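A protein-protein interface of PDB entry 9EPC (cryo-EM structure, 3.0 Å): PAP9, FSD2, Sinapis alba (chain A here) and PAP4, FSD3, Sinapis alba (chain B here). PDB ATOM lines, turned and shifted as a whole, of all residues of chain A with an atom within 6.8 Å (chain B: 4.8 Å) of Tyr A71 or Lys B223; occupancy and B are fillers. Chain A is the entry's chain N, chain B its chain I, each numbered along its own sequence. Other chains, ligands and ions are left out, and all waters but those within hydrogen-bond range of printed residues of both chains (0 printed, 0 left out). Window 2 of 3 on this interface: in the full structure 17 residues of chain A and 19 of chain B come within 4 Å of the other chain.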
ATOM      1  N   ARG A  66     -27.444 -30.699 -21.620  1.00  0.00           N
ATOM      2  CA  ARG A  66     -28.466 -31.082 -20.652  1.00  0.00           C
ATOM      3  C   ARG A  66     -28.100 -30.636 -19.241  1.00  0.00           C
ATOM      4  O   ARG A  66     -28.981 -30.250 -18.465  1.00  0.00           O
ATOM      5  CB  ARG A  66     -28.694 -32.596 -20.695  1.00  0.00           C
ATOM      6  CG  ARG A  66     -27.447 -33.419 -20.419  1.00  0.00           C
ATOM      7  CD  ARG A  66     -27.747 -34.906 -20.393  1.00  0.00           C
ATOM      8  NE  ARG A  66     -28.546 -35.287 -19.236  1.00  0.00           N
ATOM      9  CZ  ARG A  66     -29.856 -35.493 -19.262  1.00  0.00           C
ATOM     10  NH1 ARG A  66     -30.555 -35.353 -20.376  1.00  0.00           N
ATOM     11  NH2 ARG A  66     -30.476 -35.857 -18.144  1.00  0.00           N
ATOM     12  N   GLU A  67     -26.814 -30.698 -18.879  1.00  0.00           N
ATOM     13  CA  GLU A  67     -26.422 -30.312 -17.526  1.00  0.00           C
ATOM     14  C   GLU A  67     -26.673 -28.835 -17.282  1.00  0.00           C
ATOM     15  O   GLU A  67     -26.975 -28.435 -16.151  1.00  0.00           O
ATOM     16  CB  GLU A  67     -24.954 -30.662 -17.269  1.00  0.00           C
ATOM     17  CG  GLU A  67     -23.955 -29.980 -18.189  1.00  0.00           C
ATOM     18  CD  GLU A  67     -23.776 -30.707 -19.505  1.00  0.00           C
ATOM     19  OE1 GLU A  67     -24.596 -31.598 -19.813  1.00  0.00           O
ATOM     20  OE2 GLU A  67     -22.812 -30.387 -20.231  1.00  0.00           O
ATOM     21  N   THR A  68     -26.563 -28.012 -18.324  1.00  0.00           N
ATOM     22  CA  THR A  68     -27.033 -26.638 -18.221  1.00  0.00           C
ATOM     23  C   THR A  68     -28.532 -26.608 -17.964  1.00  0.00           C
ATOM     24  O   THR A  68     -29.016 -25.853 -17.114  1.00  0.00           O
ATOM     25  CB  THR A  68     -26.686 -25.872 -19.497  1.00  0.00           C
ATOM     26  OG1 THR A  68     -27.068 -26.650 -20.638  1.00  0.00           O
ATOM     27  CG2 THR A  68     -25.197 -25.596 -19.557  1.00  0.00           C
ATOM     28  N   LEU A  69     -29.282 -27.447 -18.680  1.00  0.00           N
ATOM     29  CA  LEU A  69     -30.725 -27.505 -18.482  1.00  0.00           C
ATOM     30  C   LEU A  69     -31.084 -28.142 -17.145  1.00  0.00           C
ATOM     31  O   LEU A  69     -32.155 -27.861 -16.594  1.00  0.00           O
ATOM     32  CB  LEU A  69     -31.379 -28.265 -19.636  1.00  0.00           C
ATOM     33  CG  LEU A  69     -32.889 -28.079 -19.775  1.00  0.00           C
ATOM     34  CD1 LEU A  69     -33.238 -26.611 -19.648  1.00  0.00           C
ATOM     35  CD2 LEU A  69     -33.372 -28.628 -21.104  1.00  0.00           C
ATOM     36  N   ASP A  70     -30.204 -28.990 -16.602  1.00  0.00           N
ATOM     37  CA  ASP A  70     -30.466 -29.589 -15.297  1.00  0.00           C
ATOM     38  C   ASP A  70     -30.526 -28.538 -14.200  1.00  0.00           C
ATOM     39  O   ASP A  70     -31.181 -28.750 -13.172  1.00  0.00           O
ATOM     40  CB  ASP A  70     -29.400 -30.632 -14.968  1.00  0.00           C
ATOM     41  CG  ASP A  70     -29.412 -31.799 -15.929  1.00  0.00           C
ATOM     42  OD1 ASP A  70     -30.453 -32.016 -16.583  1.00  0.00           O
ATOM     43  OD2 ASP A  70     -28.384 -32.498 -16.033  1.00  0.00           O
ATOM     44  N   TYR A  71     -29.845 -27.411 -14.387  1.00  0.00           N
ATOM     45  CA  TYR A  71     -29.904 -26.316 -13.430  1.00  0.00           C
ATOM     46  C   TYR A  71     -30.795 -25.176 -13.890  1.00  0.00           C
ATOM     47  O   TYR A  71     -31.440 -24.534 -13.055  1.00  0.00           O
ATOM     48  CB  TYR A  71     -28.499 -25.769 -13.153  1.00  0.00           C
ATOM     49  CG  TYR A  71     -27.543 -26.765 -12.535  1.00  0.00           C
ATOM     50  CD1 TYR A  71     -27.993 -27.981 -12.037  1.00  0.00           C
ATOM     51  CD2 TYR A  71     -26.189 -26.482 -12.444  1.00  0.00           C
ATOM     52  CE1 TYR A  71     -27.117 -28.888 -11.473  1.00  0.00           C
ATOM     53  CE2 TYR A  71     -25.309 -27.381 -11.881  1.00  0.00           C
ATOM     54  CZ  TYR A  71     -25.776 -28.581 -11.396  1.00  0.00           C
ATOM     55  OH  TYR A  71     -24.893 -29.475 -10.836  1.00  0.00           O
ATOM     56  N   HIS A  72     -30.847 -24.913 -15.196  1.00  0.00           N
ATOM     57  CA  HIS A  72     -31.722 -23.862 -15.702  1.00  0.00           C
ATOM     58  C   HIS A  72     -33.184 -24.191 -15.435  1.00  0.00           C
ATOM     59  O   HIS A  72     -33.967 -23.317 -15.048  1.00  0.00           O
ATOM     60  CB  HIS A  72     -31.480 -23.658 -17.197  1.00  0.00           C
ATOM     61  CG  HIS A  72     -32.152 -22.445 -17.756  1.00  0.00           C
ATOM     62  ND1 HIS A  72     -32.236 -22.198 -19.109  1.00  0.00           N
ATOM     63  CD2 HIS A  72     -32.767 -21.406 -17.146  1.00  0.00           C
ATOM     64  CE1 HIS A  72     -32.877 -21.060 -19.308  1.00  0.00           C
ATOM     65  NE2 HIS A  72     -33.207 -20.558 -18.132  1.00  0.00           N
ATOM     66  N   TRP A  73     -33.571 -25.449 -15.634  1.00  0.00           N
ATOM     67  CA  TRP A  73     -34.935 -25.893 -15.390  1.00  0.00           C
ATOM     68  C   TRP A  73     -35.089 -26.637 -14.071  1.00  0.00           C
ATOM     69  O   TRP A  73     -36.046 -26.387 -13.334  1.00  0.00           O
ATOM     70  CB  TRP A  73     -35.411 -26.792 -16.534  1.00  0.00           C
ATOM     71  CG  TRP A  73     -36.805 -27.304 -16.357  1.00  0.00           C
ATOM     72  CD1 TRP A  73     -37.957 -26.691 -16.748  1.00  0.00           C
ATOM     73  CD2 TRP A  73     -37.195 -28.538 -15.743  1.00  0.00           C
ATOM     74  NE1 TRP A  73     -39.042 -27.466 -16.418  1.00  0.00           N
ATOM     75  CE2 TRP A  73     -38.601 -28.605 -15.799  1.00  0.00           C
ATOM     76  CE3 TRP A  73     -36.492 -29.592 -15.153  1.00  0.00           C
ATOM     77  CZ2 TRP A  73     -39.317 -29.683 -15.287  1.00  0.00           C
ATOM     78  CZ3 TRP A  73     -37.206 -30.661 -14.645  1.00  0.00           C
ATOM     79  CH2 TRP A  73     -38.603 -30.699 -14.715  1.00  0.00           C
ATOM     80  N   GLY A  74     -34.167 -27.548 -13.758  1.00  0.00           N
ATOM     81  CA  GLY A  74     -34.284 -28.331 -12.543  1.00  0.00           C
ATOM     82  C   GLY A  74     -33.985 -27.564 -11.273  1.00  0.00           C
ATOM     83  O   GLY A  74     -34.449 -27.961 -10.200  1.00  0.00           O
ATOM     84  N   LYS A  75     -33.222 -26.476 -11.364  1.00  0.00           N
ATOM     85  CA  LYS A  75     -32.857 -25.692 -10.193  1.00  0.00           C
ATOM     86  C   LYS A  75     -33.464 -24.296 -10.222  1.00  0.00           C
ATOM     87  O   LYS A  75     -34.164 -23.908  -9.283  1.00  0.00           O
ATOM     88  CB  LYS A  75     -31.331 -25.606 -10.071  1.00  0.00           C
ATOM     89  CG  LYS A  75     -30.646 -26.949  -9.915  1.00  0.00           C
ATOM     90  CD  LYS A  75     -31.091 -27.649  -8.647  1.00  0.00           C
ATOM     91  CE  LYS A  75     -30.362 -28.969  -8.467  1.00  0.00           C
ATOM     92  NZ  LYS A  75     -30.758 -29.648  -7.205  1.00  0.00           N
ATOM     93  N   HIS A  76     -33.212 -23.525 -11.281  1.00  0.00           N
ATOM     94  CA  HIS A  76     -33.716 -22.156 -11.334  1.00  0.00           C
ATOM     95  C   HIS A  76     -35.238 -22.127 -11.389  1.00  0.00           C
ATOM     96  O   HIS A  76     -35.882 -21.401 -10.624  1.00  0.00           O
ATOM     97  CB  HIS A  76     -33.124 -21.423 -12.536  1.00  0.00           C
ATOM     98  CG  HIS A  76     -31.690 -21.032 -12.359  1.00  0.00           C
ATOM     99  ND1 HIS A  76     -31.309 -19.902 -11.668  1.00  0.00           N
ATOM    100  CD2 HIS A  76     -30.547 -21.617 -12.785  1.00  0.00           C
ATOM    101  CE1 HIS A  76     -29.992 -19.808 -11.675  1.00  0.00           C
ATOM    102  NE2 HIS A  76     -29.505 -20.838 -12.344  1.00  0.00           N
ATOM    103  N   HIS A  77     -35.831 -22.917 -12.284  1.00  0.00           N
ATOM    104  CA  HIS A  77     -37.281 -22.884 -12.431  1.00  0.00           C
ATOM    105  C   HIS A  77     -37.984 -23.518 -11.238  1.00  0.00           C
ATOM    106  O   HIS A  77     -39.078 -23.081 -10.865  1.00  0.00           O
ATOM    107  CB  HIS A  77     -37.698 -23.580 -13.723  1.00  0.00           C
ATOM    108  CG  HIS A  77     -38.942 -23.016 -14.332  1.00  0.00           C
ATOM    109  ND1 HIS A  77     -39.610 -23.632 -15.368  1.00  0.00           N
ATOM    110  CD2 HIS A  77     -39.636 -21.886 -14.057  1.00  0.00           C
ATOM    111  CE1 HIS A  77     -40.664 -22.910 -15.702  1.00  0.00           C
ATOM    112  NE2 HIS A  77     -40.703 -21.845 -14.922  1.00  0.00           N
ATOM    113  N   LYS A  78     -37.381 -24.543 -10.630  1.00  0.00           N
ATOM    114  CA  LYS A  78     -37.986 -25.157  -9.453  1.00  0.00           C
ATOM    115  C   LYS A  78     -38.077 -24.167  -8.301  1.00  0.00           C
ATOM    116  O   LYS A  78     -39.095 -24.109  -7.603  1.00  0.00           O
ATOM    117  CB  LYS A  78     -37.195 -26.393  -9.029  1.00  0.00           C
ATOM    118  CG  LYS A  78     -37.716 -27.691  -9.614  1.00  0.00           C
ATOM    119  CD  LYS A  78     -37.214 -28.890  -8.829  1.00  0.00           C
ATOM    120  CE  LYS A  78     -37.799 -30.184  -9.368  1.00  0.00           C
ATOM    121  NZ  LYS A  78     -37.325 -31.368  -8.599  1.00  0.00           N
ATOM    122  N   HIS A 227     -27.442 -17.206 -16.248  1.00  0.00           N
ATOM    123  CA  HIS A 227     -27.586 -18.606 -15.863  1.00  0.00           C
ATOM    124  C   HIS A 227     -28.047 -19.466 -17.030  1.00  0.00           C
ATOM    125  O   HIS A 227     -27.768 -20.670 -17.063  1.00  0.00           O
ATOM    126  CB  HIS A 227     -28.563 -18.737 -14.694  1.00  0.00           C
ATOM    127  CG  HIS A 227     -29.975 -18.374 -15.039  1.00  0.00           C
ATOM    128  ND1 HIS A 227     -30.790 -19.187 -15.797  1.00  0.00           N
ATOM    129  CD2 HIS A 227     -30.719 -17.290 -14.718  1.00  0.00           C
ATOM    130  CE1 HIS A 227     -31.973 -18.614 -15.936  1.00  0.00           C
ATOM    131  NE2 HIS A 227     -31.957 -17.463 -15.290  1.00  0.00           N
ATOM    132  N   LEU A 231     -22.967 -21.356 -18.444  1.00  0.00           N
ATOM    133  CA  LEU A 231     -22.318 -22.564 -17.949  1.00  0.00           C
ATOM    134  C   LEU A 231     -21.607 -23.337 -19.051  1.00  0.00           C
ATOM    135  O   LEU A 231     -20.542 -23.915 -18.803  1.00  0.00           O
ATOM    136  CB  LEU A 231     -23.343 -23.454 -17.248  1.00  0.00           C
ATOM    137  CG  LEU A 231     -22.807 -24.690 -16.524  1.00  0.00           C
ATOM    138  CD1 LEU A 231     -21.702 -24.309 -15.553  1.00  0.00           C
ATOM    139  CD2 LEU A 231     -23.933 -25.402 -15.798  1.00  0.00           C
ATOM    140  N   TYR B 218     -19.987 -16.478 -10.247  1.00  0.00           N
ATOM    141  CA  TYR B 218     -20.057 -17.662  -9.402  1.00  0.00           C
ATOM    142  C   TYR B 218     -20.632 -18.898 -10.073  1.00  0.00           C
ATOM    143  O   TYR B 218     -20.546 -19.978  -9.481  1.00  0.00           O
ATOM    144  CB  TYR B 218     -20.883 -17.363  -8.142  1.00  0.00           C
ATOM    145  CG  TYR B 218     -22.296 -16.905  -8.424  1.00  0.00           C
ATOM    146  CD1 TYR B 218     -23.329 -17.821  -8.571  1.00  0.00           C
ATOM    147  CD2 TYR B 218     -22.598 -15.556  -8.535  1.00  0.00           C
ATOM    148  CE1 TYR B 218     -24.620 -17.407  -8.828  1.00  0.00           C
ATOM    149  CE2 TYR B 218     -23.888 -15.133  -8.790  1.00  0.00           C
ATOM    150  CZ  TYR B 218     -24.894 -16.062  -8.935  1.00  0.00           C
ATOM    151  OH  TYR B 218     -26.180 -15.645  -9.190  1.00  0.00           O
ATOM    152  N   TYR B 219     -21.220 -18.792 -11.266  1.00  0.00           N
ATOM    153  CA  TYR B 219     -21.950 -19.928 -11.820  1.00  0.00           C
ATOM    154  C   TYR B 219     -21.019 -21.086 -12.159  1.00  0.00           C
ATOM    155  O   TYR B 219     -21.372 -22.251 -11.949  1.00  0.00           O
ATOM    156  CB  TYR B 219     -22.744 -19.501 -13.051  1.00  0.00           C
ATOM    157  CG  TYR B 219     -24.030 -20.270 -13.205  1.00  0.00           C
ATOM    158  CD1 TYR B 219     -25.161 -19.908 -12.490  1.00  0.00           C
ATOM    159  CD2 TYR B 219     -24.113 -21.365 -14.052  1.00  0.00           C
ATOM    160  CE1 TYR B 219     -26.339 -20.608 -12.618  1.00  0.00           C
ATOM    161  CE2 TYR B 219     -25.289 -22.072 -14.188  1.00  0.00           C
ATOM    162  CZ  TYR B 219     -26.400 -21.688 -13.468  1.00  0.00           C
ATOM    163  OH  TYR B 219     -27.578 -22.385 -13.596  1.00  0.00           O
ATOM    164  N   LEU B 220     -19.831 -20.791 -12.684  1.00  0.00           N
ATOM    165  CA  LEU B 220     -18.909 -21.859 -13.049  1.00  0.00           C
ATOM    166  C   LEU B 220     -18.377 -22.622 -11.843  1.00  0.00           C
ATOM    167  O   LEU B 220     -17.815 -23.707 -12.021  1.00  0.00           O
ATOM    168  CB  LEU B 220     -17.742 -21.297 -13.859  1.00  0.00           C
ATOM    169  CG  LEU B 220     -18.110 -20.701 -15.219  1.00  0.00           C
ATOM    170  CD1 LEU B 220     -16.863 -20.269 -15.973  1.00  0.00           C
ATOM    171  CD2 LEU B 220     -18.923 -21.688 -16.040  1.00  0.00           C
ATOM    172  N   ASP B 221     -18.537 -22.091 -10.633  1.00  0.00           N
ATOM    173  CA  ASP B 221     -18.068 -22.759  -9.426  1.00  0.00           C
ATOM    174  C   ASP B 221     -19.198 -23.127  -8.480  1.00  0.00           C
ATOM    175  O   ASP B 221     -19.187 -24.222  -7.906  1.00  0.00           O
ATOM    176  CB  ASP B 221     -17.042 -21.876  -8.698  1.00  0.00           C
ATOM    177  CG  ASP B 221     -15.734 -21.755  -9.455  1.00  0.00           C
ATOM    178  OD1 ASP B 221     -15.618 -22.355 -10.543  1.00  0.00           O
ATOM    179  OD2 ASP B 221     -14.820 -21.060  -8.962  1.00  0.00           O
ATOM    180  N   TYR B 222     -20.180 -22.246  -8.297  1.00  0.00           N
ATOM    181  CA  TYR B 222     -21.259 -22.477  -7.348  1.00  0.00           C
ATOM    182  C   TYR B 222     -22.626 -22.573  -8.006  1.00  0.00           C
ATOM    183  O   TYR B 222     -23.595 -22.937  -7.332  1.00  0.00           O
ATOM    184  CB  TYR B 222     -21.267 -21.372  -6.285  1.00  0.00           C
ATOM    185  CG  TYR B 222     -19.956 -21.256  -5.541  1.00  0.00           C
ATOM    186  CD1 TYR B 222     -18.943 -20.430  -6.006  1.00  0.00           C
ATOM    187  CD2 TYR B 222     -19.728 -21.983  -4.381  1.00  0.00           C
ATOM    188  CE1 TYR B 222     -17.741 -20.325  -5.334  1.00  0.00           C
ATOM    189  CE2 TYR B 222     -18.530 -21.884  -3.700  1.00  0.00           C
ATOM    190  CZ  TYR B 222     -17.541 -21.053  -4.182  1.00  0.00           C
ATOM    191  OH  TYR B 222     -16.343 -20.951  -3.511  1.00  0.00           O
ATOM    192  N   LYS B 223     -22.728 -22.269  -9.301  1.00  0.00           N
ATOM    193  CA  LYS B 223     -23.966 -22.407 -10.061  1.00  0.00           C
ATOM    194  C   LYS B 223     -25.138 -21.713  -9.378  1.00  0.00           C
ATOM    195  O   LYS B 223     -25.187 -20.482  -9.315  1.00  0.00           O
ATOM    196  CB  LYS B 223     -24.293 -23.887 -10.285  1.00  0.00           C
ATOM    197  CG  LYS B 223     -23.303 -24.631 -11.171  1.00  0.00           C
ATOM    198  CD  LYS B 223     -22.097 -25.131 -10.390  1.00  0.00           C
ATOM    199  CE  LYS B 223     -21.084 -25.794 -11.305  1.00  0.00           C
ATOM    200  NZ  LYS B 223     -20.595 -24.858 -12.353  1.00  0.00           N
ATOM    201  N   ASN B 224     -26.081 -22.497  -8.861  1.00  0.00           N
ATOM    202  CA  ASN B 224     -27.250 -21.959  -8.180  1.00  0.00           C
ATOM    203  C   ASN B 224     -27.024 -21.730  -6.694  1.00  0.00           C
ATOM    204  O   ASN B 224     -27.881 -21.124  -6.042  1.00  0.00           O
ATOM    205  CB  ASN B 224     -28.448 -22.895  -8.365  1.00  0.00           C
ATOM    206  CG  ASN B 224     -29.094 -22.751  -9.723  1.00  0.00           C
ATOM    207  OD1 ASN B 224     -30.186 -22.198  -9.844  1.00  0.00           O
ATOM    208  ND2 ASN B 224     -28.421 -23.241 -10.756  1.00  0.00           N
ATOM    209  N   GLU B 225     -25.904 -22.193  -6.145  1.00  0.00           N
ATOM    210  CA  GLU B 225     -25.643 -22.081  -4.712  1.00  0.00           C
ATOM    211  C   GLU B 225     -24.978 -20.739  -4.396  1.00  0.00           C
ATOM    212  O   GLU B 225     -23.819 -20.657  -3.991  1.00  0.00           O
ATOM    213  CB  GLU B 225     -24.787 -23.250  -4.244  1.00  0.00           C
ATOM    214  CG  GLU B 225     -25.068 -24.557  -4.972  1.00  0.00           C
ATOM    215  CD  GLU B 225     -26.507 -25.014  -4.833  1.00  0.00           C
ATOM    216  OE1 GLU B 225     -27.111 -24.772  -3.767  1.00  0.00           O
ATOM    217  OE2 GLU B 225     -27.033 -25.614  -5.793  1.00  0.00           O
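The backbone NH of His A76 is in hydrogen-bond range of the backbone carbonyl oxygen of Tyr A71, 2.7 Å away. O of Tyr B218 lies within hydrogen-bond range of N of Lys B223, at 3.2 Å. The backbone carbonyl oxygen of Tyr B219 lies within hydrogen-bond range of the side-chain amino group of Lys B223, 2.8 Å away. The side-chain hydroxyl of Tyr B219 is in hydrogen-bond range of the side-chain amide nitrogen of Asn B224 (3.1 Å). NZ of Lys B223 lies within hydrogen-bond range of O of Leu B220, at 3.0 Å.
Tyr A71 touches just these residues of chain B: Tyr B219 (3.5 Å), Lys B223 (3.5 Å) and Asn B224 (3.5 Å). Of chain A, only Tyr A71 and Leu A231 come within 4 Å of Lys B223. Of the printed residues of chain A, Tyr B219 touches Tyr A71 (3.5 Å), His A76 (2.8 Å), His A227 (3.6 Å) and Leu A231 (3.9 Å). Of the printed residues of chain A, Leu B220 touches Leu A231. Of the printed residues of chain B, Leu A231 touches Tyr B219 (3.9 Å), Leu B220 (3.9 Å) and Lys B223 (3.4 Å). Printed residues of chain B within 4 Å of Lys A75: Asn B224 (3.6 Å). Asp B221 touches none of the printed residues of chain A. The nearest printed residue of chain B that does not touch His A76 is Lys B223 (5.3 Å).
Among the printed residues, merely in contact across the chains: Tyr A71 with Tyr B219 (3.5 Å), Tyr A71 with Lys B223 (3.5 Å), Tyr A71 with Asn B224 (3.5 Å), Lys A75 with Asn B224 (3.6 Å), His A227 with Tyr B219 (3.6 Å), Leu A231 with Tyr B219 (3.9 Å), Leu A231 with Leu B220 (3.9 Å) and Leu A231 with Lys B223 (3.4 Å).
NE2 of His A76 is in hydrogen-bond range of OH of Tyr B219 (2.8 Å). A ring nitrogen (NE2) of His A76 sits at hydrogen-bond distance from the side-chain amide oxygen (OD1) of Asn B224, at 2.9 Å.
Hydrophobic or aromatic side chains of chain A within 4 Å of the printed part of chain B: Tyr A71, His A76, His A227 and Leu A231. Hydrophobic or aromatic side chains of chain B within 4 Å of the printed part of chain A: Tyr B219 and Leu B220. Among the printed residues, no Asp or Glu carboxylate lies within 4 Å of a Lys or Arg side-chain nitrogen of the other chain.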
